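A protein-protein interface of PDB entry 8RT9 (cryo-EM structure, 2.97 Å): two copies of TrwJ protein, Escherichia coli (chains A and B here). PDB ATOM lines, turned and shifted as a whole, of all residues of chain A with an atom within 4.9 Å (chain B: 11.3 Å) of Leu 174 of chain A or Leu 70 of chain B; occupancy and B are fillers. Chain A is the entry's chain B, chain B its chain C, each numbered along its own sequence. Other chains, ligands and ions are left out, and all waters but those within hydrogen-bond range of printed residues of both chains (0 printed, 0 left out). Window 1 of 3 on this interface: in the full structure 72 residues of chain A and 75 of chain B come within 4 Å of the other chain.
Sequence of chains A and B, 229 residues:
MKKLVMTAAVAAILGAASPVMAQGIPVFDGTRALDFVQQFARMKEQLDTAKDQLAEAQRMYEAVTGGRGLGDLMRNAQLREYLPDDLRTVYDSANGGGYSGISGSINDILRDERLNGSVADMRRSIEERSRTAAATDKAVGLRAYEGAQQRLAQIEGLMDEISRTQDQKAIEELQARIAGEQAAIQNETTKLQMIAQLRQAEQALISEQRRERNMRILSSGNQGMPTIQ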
ATOM      1  N   LEU A 158      25.495 -11.268  26.647  1.00  0.00           N
ATOM      2  CA  LEU A 158      25.036 -11.952  25.405  1.00  0.00           C
ATOM      3  C   LEU A 158      23.592 -12.438  25.593  1.00  0.00           C
ATOM      4  O   LEU A 158      22.801 -12.317  24.637  1.00  0.00           O
ATOM      5  CB  LEU A 158      25.980 -13.114  25.081  1.00  0.00           C
ATOM      6  CG  LEU A 158      27.369 -12.708  24.593  1.00  0.00           C
ATOM      7  CD1 LEU A 158      28.226 -13.935  24.323  1.00  0.00           C
ATOM      8  CD2 LEU A 158      27.276 -11.842  23.346  1.00  0.00           C
ATOM      9  N   GLU A 161      21.003  -9.735  25.133  1.00  0.00           N
ATOM     10  CA  GLU A 161      20.710  -9.537  23.687  1.00  0.00           C
ATOM     11  C   GLU A 161      19.700 -10.590  23.220  1.00  0.00           C
ATOM     12  O   GLU A 161      18.853 -10.255  22.372  1.00  0.00           O
ATOM     13  CB  GLU A 161      22.004  -9.587  22.872  1.00  0.00           C
ATOM     14  CG  GLU A 161      21.820  -9.231  21.408  1.00  0.00           C
ATOM     15  CD  GLU A 161      21.629  -7.752  21.117  1.00  0.00           C
ATOM     16  OE1 GLU A 161      22.022  -6.926  21.966  1.00  0.00           O
ATOM     17  OE2 GLU A 161      21.084  -7.431  20.044  1.00  0.00           O
ATOM     18  N   ILE A 162      19.780 -11.813  23.753  1.00  0.00           N
ATOM     19  CA  ILE A 162      18.897 -12.924  23.279  1.00  0.00           C
ATOM     20  C   ILE A 162      17.427 -12.540  23.491  1.00  0.00           C
ATOM     21  O   ILE A 162      16.598 -12.901  22.632  1.00  0.00           O
ATOM     22  CB  ILE A 162      19.289 -14.266  23.938  1.00  0.00           C
ATOM     23  CG1 ILE A 162      20.677 -14.728  23.495  1.00  0.00           C
ATOM     24  CG2 ILE A 162      18.260 -15.356  23.682  1.00  0.00           C
ATOM     25  CD1 ILE A 162      21.194 -15.882  24.310  1.00  0.00           C
ATOM     26  N   THR A 165      15.986 -10.258  20.604  1.00  0.00           N
ATOM     27  CA  THR A 165      16.130 -10.688  19.183  1.00  0.00           C
ATOM     28  C   THR A 165      14.762 -10.683  18.493  1.00  0.00           C
ATOM     29  O   THR A 165      13.778 -11.097  19.140  1.00  0.00           O
ATOM     30  CB  THR A 165      16.826 -12.049  19.064  1.00  0.00           C
ATOM     31  OG1 THR A 165      16.150 -12.973  19.916  1.00  0.00           O
ATOM     32  CG2 THR A 165      18.294 -11.984  19.423  1.00  0.00           C
ATOM     33  N   ALA A 170      18.714 -12.590  12.975  1.00  0.00           N
ATOM     34  CA  ALA A 170      19.329 -12.015  14.162  1.00  0.00           C
ATOM     35  C   ALA A 170      19.633 -13.086  15.199  1.00  0.00           C
ATOM     36  O   ALA A 170      20.734 -13.133  15.759  1.00  0.00           O
ATOM     37  CB  ALA A 170      18.418 -10.941  14.748  1.00  0.00           C
ATOM     38  N   ILE A 171      18.669 -13.967  15.463  1.00  0.00           N
ATOM     39  CA  ILE A 171      18.888 -14.980  16.486  1.00  0.00           C
ATOM     40  C   ILE A 171      19.885 -16.026  16.012  1.00  0.00           C
ATOM     41  O   ILE A 171      20.631 -16.584  16.822  1.00  0.00           O
ATOM     42  CB  ILE A 171      17.554 -15.607  16.928  1.00  0.00           C
ATOM     43  CG1 ILE A 171      17.760 -16.478  18.161  1.00  0.00           C
ATOM     44  CG2 ILE A 171      16.947 -16.410  15.826  1.00  0.00           C
ATOM     45  CD1 ILE A 171      18.298 -15.728  19.342  1.00  0.00           C
ATOM     46  N   GLU A 172      19.937 -16.311  14.711  1.00  0.00           N
ATOM     47  CA  GLU A 172      20.954 -17.238  14.225  1.00  0.00           C
ATOM     48  C   GLU A 172      22.354 -16.646  14.357  1.00  0.00           C
ATOM     49  O   GLU A 172      23.297 -17.343  14.762  1.00  0.00           O
ATOM     50  CB  GLU A 172      20.646 -17.639  12.786  1.00  0.00           C
ATOM     51  CG  GLU A 172      19.465 -18.589  12.687  1.00  0.00           C
ATOM     52  CD  GLU A 172      19.130 -18.981  11.266  1.00  0.00           C
ATOM     53  OE1 GLU A 172      19.660 -18.349  10.331  1.00  0.00           O
ATOM     54  OE2 GLU A 172      18.339 -19.928  11.084  1.00  0.00           O
ATOM     55  N   GLU A 173      22.508 -15.358  14.049  1.00  0.00           N
ATOM     56  CA  GLU A 173      23.794 -14.710  14.284  1.00  0.00           C
ATOM     57  C   GLU A 173      24.150 -14.714  15.760  1.00  0.00           C
ATOM     58  O   GLU A 173      25.316 -14.896  16.120  1.00  0.00           O
ATOM     59  CB  GLU A 173      23.790 -13.281  13.750  1.00  0.00           C
ATOM     60  CG  GLU A 173      23.633 -13.167  12.258  1.00  0.00           C
ATOM     61  CD  GLU A 173      24.090 -11.822  11.747  1.00  0.00           C
ATOM     62  OE1 GLU A 173      24.468 -10.978  12.583  1.00  0.00           O
ATOM     63  OE2 GLU A 173      24.080 -11.603  10.518  1.00  0.00           O
ATOM     64  N   LEU A 174      23.167 -14.512  16.632  1.00  0.00           N
ATOM     65  CA  LEU A 174      23.466 -14.537  18.058  1.00  0.00           C
ATOM     66  C   LEU A 174      23.875 -15.928  18.514  1.00  0.00           C
ATOM     67  O   LEU A 174      24.753 -16.070  19.371  1.00  0.00           O
ATOM     68  CB  LEU A 174      22.271 -14.044  18.858  1.00  0.00           C
ATOM     69  CG  LEU A 174      22.595 -13.737  20.310  1.00  0.00           C
ATOM     70  CD1 LEU A 174      23.895 -12.979  20.401  1.00  0.00           C
ATOM     71  CD2 LEU A 174      21.490 -12.910  20.871  1.00  0.00           C
ATOM     72  N   GLN A 175      23.248 -16.967  17.964  1.00  0.00           N
ATOM     73  CA  GLN A 175      23.656 -18.324  18.301  1.00  0.00           C
ATOM     74  C   GLN A 175      25.093 -18.577  17.888  1.00  0.00           C
ATOM     75  O   GLN A 175      25.869 -19.170  18.646  1.00  0.00           O
ATOM     76  CB  GLN A 175      22.738 -19.345  17.638  1.00  0.00           C
ATOM     77  CG  GLN A 175      21.390 -19.479  18.285  1.00  0.00           C
ATOM     78  CD  GLN A 175      20.468 -20.378  17.508  1.00  0.00           C
ATOM     79  OE1 GLN A 175      20.906 -21.341  16.886  1.00  0.00           O
ATOM     80  NE2 GLN A 175      19.180 -20.070  17.535  1.00  0.00           N
ATOM     81  N   ALA A 176      25.471 -18.137  16.691  1.00  0.00           N
ATOM     82  CA  ALA A 176      26.844 -18.359  16.255  1.00  0.00           C
ATOM     83  C   ALA A 176      27.828 -17.525  17.072  1.00  0.00           C
ATOM     84  O   ALA A 176      28.953 -17.963  17.341  1.00  0.00           O
ATOM     85  CB  ALA A 176      26.975 -18.082  14.763  1.00  0.00           C
ATOM     86  N   ARG A 177      27.418 -16.330  17.497  1.00  0.00           N
ATOM     87  CA  ARG A 177      28.254 -15.536  18.390  1.00  0.00           C
ATOM     88  C   ARG A 177      28.473 -16.235  19.724  1.00  0.00           C
ATOM     89  O   ARG A 177      29.597 -16.276  20.237  1.00  0.00           O
ATOM     90  CB  ARG A 177      27.626 -14.164  18.607  1.00  0.00           C
ATOM     91  CG  ARG A 177      28.357 -13.311  19.609  1.00  0.00           C
ATOM     92  CD  ARG A 177      29.703 -12.868  19.114  1.00  0.00           C
ATOM     93  NE  ARG A 177      30.333 -11.968  20.068  1.00  0.00           N
ATOM     94  CZ  ARG A 177      31.096 -12.369  21.076  1.00  0.00           C
ATOM     95  NH1 ARG A 177      31.628 -11.482  21.898  1.00  0.00           N
ATOM     96  NH2 ARG A 177      31.323 -13.657  21.266  1.00  0.00           N
ATOM     97  N   ILE A 178      27.413 -16.799  20.301  1.00  0.00           N
ATOM     98  CA  ILE A 178      27.558 -17.507  21.567  1.00  0.00           C
ATOM     99  C   ILE A 178      28.413 -18.754  21.383  1.00  0.00           C
ATOM    100  O   ILE A 178      29.178 -19.137  22.276  1.00  0.00           O
ATOM    101  CB  ILE A 178      26.176 -17.837  22.153  1.00  0.00           C
ATOM    102  CG1 ILE A 178      25.411 -16.550  22.439  1.00  0.00           C
ATOM    103  CG2 ILE A 178      26.317 -18.629  23.426  1.00  0.00           C
ATOM    104  CD1 ILE A 178      24.075 -16.770  23.070  1.00  0.00           C
ATOM    105  N   ALA B  63      13.232 -10.610   6.448  1.00  0.00           N
ATOM    106  CA  ALA B  63      13.413 -11.120   7.800  1.00  0.00           C
ATOM    107  C   ALA B  63      14.403 -12.271   7.844  1.00  0.00           C
ATOM    108  O   ALA B  63      15.032 -12.501   8.880  1.00  0.00           O
ATOM    109  CB  ALA B  63      12.072 -11.566   8.375  1.00  0.00           C
ATOM    110  N   VAL B  64      14.548 -13.007   6.749  1.00  0.00           N
ATOM    111  CA  VAL B  64      15.447 -14.155   6.721  1.00  0.00           C
ATOM    112  C   VAL B  64      16.857 -13.759   6.298  1.00  0.00           C
ATOM    113  O   VAL B  64      17.838 -14.228   6.877  1.00  0.00           O
ATOM    114  CB  VAL B  64      14.869 -15.243   5.798  1.00  0.00           C
ATOM    115  CG1 VAL B  64      15.895 -16.318   5.537  1.00  0.00           C
ATOM    116  CG2 VAL B  64      13.624 -15.837   6.413  1.00  0.00           C
ATOM    117  N   GLY B  66      20.036 -10.918   5.014  1.00  0.00           N
ATOM    118  CA  GLY B  66      20.661  -9.673   5.399  1.00  0.00           C
ATOM    119  C   GLY B  66      21.615  -9.871   6.556  1.00  0.00           C
ATOM    120  O   GLY B  66      21.766 -10.971   7.093  1.00  0.00           O
ATOM    121  N   GLY B  67      22.269  -8.785   6.949  1.00  0.00           N
ATOM    122  CA  GLY B  67      23.160  -8.796   8.095  1.00  0.00           C
ATOM    123  C   GLY B  67      22.582  -7.992   9.241  1.00  0.00           C
ATOM    124  O   GLY B  67      22.045  -6.903   9.034  1.00  0.00           O
ATOM    125  N   ARG B  68      22.682  -8.525  10.457  1.00  0.00           N
ATOM    126  CA  ARG B  68      22.027  -7.924  11.610  1.00  0.00           C
ATOM    127  C   ARG B  68      22.999  -7.290  12.593  1.00  0.00           C
ATOM    128  O   ARG B  68      22.558  -6.660  13.558  1.00  0.00           O
ATOM    129  CB  ARG B  68      21.175  -8.964  12.332  1.00  0.00           C
ATOM    130  CG  ARG B  68      20.081  -9.545  11.477  1.00  0.00           C
ATOM    131  CD  ARG B  68      19.048  -8.509  11.139  1.00  0.00           C
ATOM    132  NE  ARG B  68      17.918  -9.104  10.444  1.00  0.00           N
ATOM    133  CZ  ARG B  68      17.847  -9.243   9.128  1.00  0.00           C
ATOM    134  NH1 ARG B  68      18.846  -8.834   8.363  1.00  0.00           N
ATOM    135  NH2 ARG B  68      16.779  -9.796   8.576  1.00  0.00           N
ATOM    136  N   GLY B  69      24.300  -7.442  12.387  1.00  0.00           N
ATOM    137  CA  GLY B  69      25.277  -6.792  13.223  1.00  0.00           C
ATOM    138  C   GLY B  69      25.671  -7.552  14.467  1.00  0.00           C
ATOM    139  O   GLY B  69      26.673  -7.202  15.093  1.00  0.00           O
ATOM    140  N   LEU B  70      24.910  -8.569  14.857  1.00  0.00           N
ATOM    141  CA  LEU B  70      25.328  -9.418  15.961  1.00  0.00           C
ATOM    142  C   LEU B  70      26.547 -10.218  15.536  1.00  0.00           C
ATOM    143  O   LEU B  70      26.598 -10.786  14.443  1.00  0.00           O
ATOM    144  CB  LEU B  70      24.193 -10.340  16.399  1.00  0.00           C
ATOM    145  CG  LEU B  70      23.048  -9.727  17.212  1.00  0.00           C
ATOM    146  CD1 LEU B  70      22.276  -8.662  16.455  1.00  0.00           C
ATOM    147  CD2 LEU B  70      22.105 -10.806  17.675  1.00  0.00           C
ATOM    148  N   GLY B  71      27.543 -10.248  16.404  1.00  0.00           N
ATOM    149  CA  GLY B  71      28.899 -10.465  15.974  1.00  0.00           C
ATOM    150  C   GLY B  71      29.575  -9.179  15.575  1.00  0.00           C
ATOM    151  O   GLY B  71      29.070  -8.496  14.679  1.00  0.00           O
ATOM    152  N   ASP B  72      30.713  -8.852  16.183  1.00  0.00           N
ATOM    153  CA  ASP B  72      31.083  -7.483  16.518  1.00  0.00           C
ATOM    154  C   ASP B  72      30.193  -6.964  17.636  1.00  0.00           C
ATOM    155  O   ASP B  72      29.891  -5.771  17.706  1.00  0.00           O
ATOM    156  CB  ASP B  72      31.033  -6.549  15.309  1.00  0.00           C
ATOM    157  CG  ASP B  72      32.117  -6.852  14.295  1.00  0.00           C
ATOM    158  OD1 ASP B  72      33.193  -7.342  14.699  1.00  0.00           O
ATOM    159  OD2 ASP B  72      31.893  -6.598  13.093  1.00  0.00           O
ATOM    160  N   LEU B  73      29.755  -7.870  18.506  1.00  0.00           N
ATOM    161  CA  LEU B  73      28.977  -7.557  19.693  1.00  0.00           C
ATOM    162  C   LEU B  73      29.763  -8.025  20.906  1.00  0.00           C
ATOM    163  O   LEU B  73      29.975  -9.229  21.081  1.00  0.00           O
ATOM    164  CB  LEU B  73      27.614  -8.241  19.647  1.00  0.00           C
ATOM    165  CG  LEU B  73      26.659  -7.898  20.781  1.00  0.00           C
ATOM    166  CD1 LEU B  73      26.099  -6.502  20.595  1.00  0.00           C
ATOM    167  CD2 LEU B  73      25.549  -8.915  20.841  1.00  0.00           C
ATOM    168  N   MET B  74      30.182  -7.077  21.739  1.00  0.00           N
ATOM    169  CA  MET B  74      31.030  -7.363  22.893  1.00  0.00           C
ATOM    170  C   MET B  74      32.303  -8.082  22.462  1.00  0.00           C
ATOM    171  O   MET B  74      32.668  -9.127  23.001  1.00  0.00           O
ATOM    172  CB  MET B  74      30.271  -8.163  23.949  1.00  0.00           C
ATOM    173  CG  MET B  74      29.102  -7.405  24.530  1.00  0.00           C
ATOM    174  SD  MET B  74      28.006  -8.412  25.533  1.00  0.00           S
ATOM    175  CE  MET B  74      27.420  -7.186  26.695  1.00  0.00           C
ATOM    176  N   ARG B  75      32.979  -7.513  21.469  1.00  0.00           N
ATOM    177  CA  ARG B  75      34.196  -8.090  20.928  1.00  0.00           C
ATOM    178  C   ARG B  75      35.446  -7.301  21.288  1.00  0.00           C
ATOM    179  O   ARG B  75      36.553  -7.828  21.151  1.00  0.00           O
ATOM    180  CB  ARG B  75      34.087  -8.204  19.407  1.00  0.00           C
ATOM    181  CG  ARG B  75      33.053  -9.210  18.950  1.00  0.00           C
ATOM    182  CD  ARG B  75      33.624 -10.610  18.896  1.00  0.00           C
ATOM    183  NE  ARG B  75      34.823 -10.685  18.076  1.00  0.00           N
ATOM    184  CZ  ARG B  75      34.835 -10.564  16.755  1.00  0.00           C
ATOM    185  NH1 ARG B  75      35.980 -10.644  16.094  1.00  0.00           N
ATOM    186  NH2 ARG B  75      33.706 -10.380  16.090  1.00  0.00           N
ATOM    187  N   LYS B 169      10.879 -19.484  16.220  1.00  0.00           N
ATOM    188  CA  LYS B 169      11.618 -18.466  16.953  1.00  0.00           C
ATOM    189  C   LYS B 169      11.804 -18.871  18.405  1.00  0.00           C
ATOM    190  O   LYS B 169      12.867 -18.639  18.990  1.00  0.00           O
ATOM    191  CB  LYS B 169      10.890 -17.132  16.849  1.00  0.00           C
ATOM    192  CG  LYS B 169      11.628 -15.969  17.449  1.00  0.00           C
ATOM    193  CD  LYS B 169      12.830 -15.609  16.625  1.00  0.00           C
ATOM    194  CE  LYS B 169      13.466 -14.345  17.146  1.00  0.00           C
ATOM    195  NZ  LYS B 169      13.495 -14.328  18.625  1.00  0.00           N
ATOM    196  N   ILE B 171      12.033 -21.950  19.709  1.00  0.00           N
ATOM    197  CA  ILE B 171      13.036 -22.991  19.882  1.00  0.00           C
ATOM    198  C   ILE B 171      14.426 -22.469  19.557  1.00  0.00           C
ATOM    199  O   ILE B 171      15.412 -22.915  20.150  1.00  0.00           O
ATOM    200  CB  ILE B 171      12.675 -24.238  19.055  1.00  0.00           C
ATOM    201  CG1 ILE B 171      13.583 -25.403  19.430  1.00  0.00           C
ATOM    202  CG2 ILE B 171      12.772 -23.960  17.591  1.00  0.00           C
ATOM    203  CD1 ILE B 171      13.490 -25.798  20.873  1.00  0.00           C
ATOM    204  N   GLU B 172      14.546 -21.516  18.632  1.00  0.00           N
ATOM    205  CA  GLU B 172      15.860 -20.932  18.377  1.00  0.00           C
ATOM    206  C   GLU B 172      16.345 -20.115  19.570  1.00  0.00           C
ATOM    207  O   GLU B 172      17.524 -20.190  19.949  1.00  0.00           O
ATOM    208  CB  GLU B 172      15.819 -20.097  17.102  1.00  0.00           C
ATOM    209  CG  GLU B 172      15.748 -20.952  15.848  1.00  0.00           C
ATOM    210  CD  GLU B 172      15.682 -20.140  14.574  1.00  0.00           C
ATOM    211  OE1 GLU B 172      15.465 -18.916  14.656  1.00  0.00           O
ATOM    212  OE2 GLU B 172      15.858 -20.730  13.488  1.00  0.00           O
ATOM    213  N   GLU B 173      15.450 -19.350  20.196  1.00  0.00           N
ATOM    214  CA  GLU B 173      15.828 -18.653  21.419  1.00  0.00           C
ATOM    215  C   GLU B 173      16.209 -19.633  22.515  1.00  0.00           C
ATOM    216  O   GLU B 173      17.144 -19.381  23.280  1.00  0.00           O
ATOM    217  CB  GLU B 173      14.702 -17.743  21.900  1.00  0.00           C
ATOM    218  CG  GLU B 173      14.368 -16.609  20.967  1.00  0.00           C
ATOM    219  CD  GLU B 173      13.609 -15.510  21.670  1.00  0.00           C
ATOM    220  OE1 GLU B 173      13.306 -15.683  22.866  1.00  0.00           O
ATOM    221  OE2 GLU B 173      13.319 -14.473  21.037  1.00  0.00           O
ATOM    222  N   LEU B 174      15.499 -20.752  22.615  1.00  0.00           N
ATOM    223  CA  LEU B 174      15.853 -21.730  23.636  1.00  0.00           C
ATOM    224  C   LEU B 174      17.208 -22.359  23.356  1.00  0.00           C
ATOM    225  O   LEU B 174      17.973 -22.631  24.287  1.00  0.00           O
ATOM    226  CB  LEU B 174      14.780 -22.801  23.738  1.00  0.00           C
ATOM    227  CG  LEU B 174      14.903 -23.671  24.977  1.00  0.00           C
ATOM    228  CD1 LEU B 174      15.195 -22.816  26.184  1.00  0.00           C
ATOM    229  CD2 LEU B 174      13.615 -24.394  25.172  1.00  0.00           C
ATOM    230  N   GLN B 175      17.522 -22.605  22.085  1.00  0.00           N
ATOM    231  CA  GLN B 175      18.840 -23.128  21.751  1.00  0.00           C
ATOM    232  C   GLN B 175      19.929 -22.156  22.156  1.00  0.00           C
ATOM    233  O   GLN B 175      20.956 -22.558  22.714  1.00  0.00           O
ATOM    234  CB  GLN B 175      18.940 -23.429  20.259  1.00  0.00           C
ATOM    235  CG  GLN B 175      18.222 -24.675  19.830  1.00  0.00           C
ATOM    236  CD  GLN B 175      18.217 -24.846  18.335  1.00  0.00           C
ATOM    237  OE1 GLN B 175      19.165 -24.465  17.655  1.00  0.00           O
ATOM    238  NE2 GLN B 175      17.145 -25.421  17.809  1.00  0.00           N
ATOM    239  N   ALA B 176      19.730 -20.868  21.884  1.00  0.00           N
ATOM    240  CA  ALA B 176      20.753 -19.898  22.257  1.00  0.00           C
ATOM    241  C   ALA B 176      20.851 -19.749  23.773  1.00  0.00           C
ATOM    242  O   ALA B 176      21.943 -19.535  24.315  1.00  0.00           O
ATOM    243  CB  ALA B 176      20.485 -18.562  21.575  1.00  0.00           C
ATOM    244  N   ARG B 177      19.729 -19.881  24.478  1.00  0.00           N
ATOM    245  CA  ARG B 177      19.768 -19.883  25.937  1.00  0.00           C
ATOM    246  C   ARG B 177      20.566 -21.061  26.476  1.00  0.00           C
ATOM    247  O   ARG B 177      21.382 -20.902  27.392  1.00  0.00           O
ATOM    248  CB  ARG B 177      18.350 -19.901  26.495  1.00  0.00           C
ATOM    249  CG  ARG B 177      18.287 -20.021  27.994  1.00  0.00           C
ATOM    250  CD  ARG B 177      18.787 -18.790  28.691  1.00  0.00           C
ATOM    251  NE  ARG B 177      18.618 -18.907  30.132  1.00  0.00           N
ATOM    252  CZ  ARG B 177      19.515 -19.448  30.944  1.00  0.00           C
ATOM    253  NH1 ARG B 177      19.279 -19.514  32.243  1.00  0.00           N
ATOM    254  NH2 ARG B 177      20.649 -19.924  30.458  1.00  0.00           N
ATOM    255  N   ILE B 178      20.351 -22.251  25.922  1.00  0.00           N
ATOM    256  CA  ILE B 178      21.100 -23.417  26.374  1.00  0.00           C
ATOM    257  C   ILE B 178      22.577 -23.265  26.033  1.00  0.00           C
ATOM    258  O   ILE B 178      23.453 -23.706  26.787  1.00  0.00           O
ATOM    259  CB  ILE B 178      20.500 -24.699  25.776  1.00  0.00           C
ATOM    260  CG1 ILE B 178      19.064 -24.873  26.252  1.00  0.00           C
ATOM    261  CG2 ILE B 178      21.311 -25.901  26.184  1.00  0.00           C
ATOM    262  CD1 ILE B 178      18.415 -26.129  25.769  1.00  0.00           C
ATOM    263  N   ALA B 179      22.881 -22.637  24.897  1.00  0.00           N
ATOM    264  CA  ALA B 179      24.274 -22.371  24.558  1.00  0.00           C
ATOM    265  C   ALA B 179      24.920 -21.438  25.572  1.00  0.00           C
ATOM    266  O   ALA B 179      26.065 -21.653  25.989  1.00  0.00           O
ATOM    267  CB  ALA B 179      24.370 -21.786  23.153  1.00  0.00           C
ATOM    268  N   GLY B 180      24.204 -20.394  25.981  1.00  0.00           N
ATOM    269  CA  GLY B 180      24.721 -19.530  27.029  1.00  0.00           C
ATOM    270  C   GLY B 180      24.916 -20.271  28.335  1.00  0.00           C
ATOM    271  O   GLY B 180      25.861 -20.005  29.084  1.00  0.00           O
ATOM    272  N   GLU B 181      24.023 -21.212  28.627  1.00  0.00           N
ATOM    273  CA  GLU B 181      24.152 -22.006  29.842  1.00  0.00           C
ATOM    274  C   GLU B 181      25.419 -22.855  29.796  1.00  0.00           C
ATOM    275  O   GLU B 181      26.151 -22.970  30.791  1.00  0.00           O
ATOM    276  CB  GLU B 181      22.917 -22.887  29.993  1.00  0.00           C
ATOM    277  CG  GLU B 181      22.846 -23.637  31.281  1.00  0.00           C
ATOM    278  CD  GLU B 181      22.683 -22.690  32.443  1.00  0.00           C
ATOM    279  OE1 GLU B 181      22.162 -21.573  32.234  1.00  0.00           O
ATOM    280  OE2 GLU B 181      23.065 -23.050  33.566  1.00  0.00           O
ATOM    281  N   ALA B 183      28.063 -22.049  28.115  1.00  0.00           N
ATOM    282  CA  ALA B 183      29.161 -21.107  28.301  1.00  0.00           C
ATOM    283  C   ALA B 183      29.391 -20.826  29.778  1.00  0.00           C
ATOM    284  O   ALA B 183      30.538 -20.712  30.228  1.00  0.00           O
ATOM    285  CB  ALA B 183      28.877 -19.814  27.545  1.00  0.00           C
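The side-chain carboxylate (OD1) of Asp 72 of chain B lies within salt-bridge range of the guanidinium group (NH2) of Arg 75 of chain B (3.4 Å). The side-chain hydroxyl (OG1) of Thr 165 of chain A is in hydrogen-bond range of the backbone carbonyl oxygen (O) of Ile 162 of chain A, 2.8 Å away. NZ of Lys 169 of chain B lies within salt-bridge range of OE2 of Glu 173 of chain B (2.4 Å). NH2 of Arg 68 of chain B is in hydrogen-bond range of O of Ala 63 of chain B (3.2 Å).
Glu 161 of chain A touches Leu 70 of chain B (OE2 to CD1, 3.98 Å). O of Ile 162 of chain A touches OE2 of Glu 173 of chain B, 3.97 Å away. O of Ala 176 of chain B touches CD1 of Ile 162 of chain A, at 3.7 Å. Ala 170 of chain A touches Leu 70 of chain B (O to CD2, 3.3 Å). Ile 171 of chain A touches Glu 172 of chain B (CG2 to OE1, 3.1 Å). Glu 172 of chain A touches Glu 172 of chain B (OE2 to OE2, 3.5 Å). NH1 of Arg 177 of chain A touches CD of Arg 75 of chain B, 3.7 Å away. O of Ala 176 of chain B touches CD1 of Ile 178 of chain A, at 3.7 Å.
Ile 171 of chain A touches Glu 172 of chain B, but with the chains exchanged Glu 172 of chain A does not touch Ile 171 of chain B (9.4 Å). Glu 172 of chain B touches its own counterpart, Glu 172 of chain A. Gln 175 of chain A touches Glu 172 of chain B, but with the chains exchanged Glu 172 of chain A does not touch Gln 175 of chain B (7.7 Å). 8 positions are printed for both chains. Of the 25 pairs that touch across the chains among the printed residues, 2 have their exchanged pair printed and touching as well.
The guanidinium group (NH1) of Arg 177 of chain A sits at hydrogen-bond distance from the backbone carbonyl oxygen (O) of Met 74 of chain B (2.8 Å). O of Glu 172 of chain B lies within hydrogen-bond range of NE2 of Gln 175 of chain A, at 2.9 Å. The side-chain amino group (NZ) of Lys 169 of chain B is in hydrogen-bond range of the side-chain hydroxyl (OG1) of Thr 165 of chain A, 3.2 Å away. N of Arg 68 of chain B is in hydrogen-bond range of OE2 of Glu 173 of chain A (3.4 Å). The side-chain carboxylate (OE1) of Glu 173 of chain A is in hydrogen-bond range of the backbone NH (N) of Leu 70 of chain B (3.3 Å). NH1 of Arg 177 of chain A is in hydrogen-bond range of O of Leu 73 of chain B (2.9 Å). OG1 of Thr 165 of chain A is in hydrogen-bond range of OE2 of Glu 173 of chain B (3.4 Å).
Leu 174 of chain A touches just one residue of chain B: Leu 70 (3.5 Å). Leu 70 of chain B touches four residues of chain A. Leu 158 of chain A touches just one residue of chain B: Met 74. Ile 162 of chain A touches just these residues of chain B: Glu 173 and Ala 176. Ala 170 of chain A touches just these residues of chain B: Arg 68 and Leu 70. Gln 175 of chain A touches just these residues of chain B: Glu 172 (2.9 Å), Gln 175 (3.7 Å) and Ala 176 (3.5 Å). Of the printed residues of chain B, Ile 178 of chain A touches Ala 176, Ala 179 and Gly 180. Printed residues of chain A within 4 Å of Gly 180 of chain B: Ile 178. Printed residues of chain A within 4 Å of Glu 173 of chain B: Ile 162 (3.97 Å) and Thr 165 (3.4 Å). Printed residues of chain A within 4 Å of Gly 67 of chain B: Glu 173 (3.8 Å). Printed residues of chain A within 4 Å of Leu 73 of chain B: Glu 161 and Arg 177. Of the printed residues of chain A, Met 74 of chain B touches Leu 158 and Arg 177. The nearest printed residue of chain A that does not touch Gly 69 of chain B is Ala 170 of chain A (7.0 Å).
Of the 13 printed residues of chain A, 12 touch a printed residue of chain B. Printed residues of chain A that touch a printed residue of chain B: Leu 158, Glu 161, Ile 162, Thr 165, Ala 170, Ile 171, Glu 172, Glu 173, Leu 174, Gln 175, Arg 177 and Ile 178. Hydrophobic or aromatic side chains of chain A within 4 Å of the printed part of chain B: Ile 162, Ala 170, Ile 171, Leu 174 and Ile 178. Along chain A the printed residues that touch a printed residue of chain B span positions 158 to 178. Of the 25 printed residues of chain B, 14 touch a printed residue of chain A. Hydrophobic or aromatic side chains of chain B within 4 Å of the printed part of chain A: Leu 70, Leu 73, Met 74, Ala 176 and Ala 179. Among the printed residues, 25 pairs touch across the chains. Among the printed residues, no Asp or Glu carboxylate lies within 4 Å of a Lys or Arg side-chain nitrogen of the other chain.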
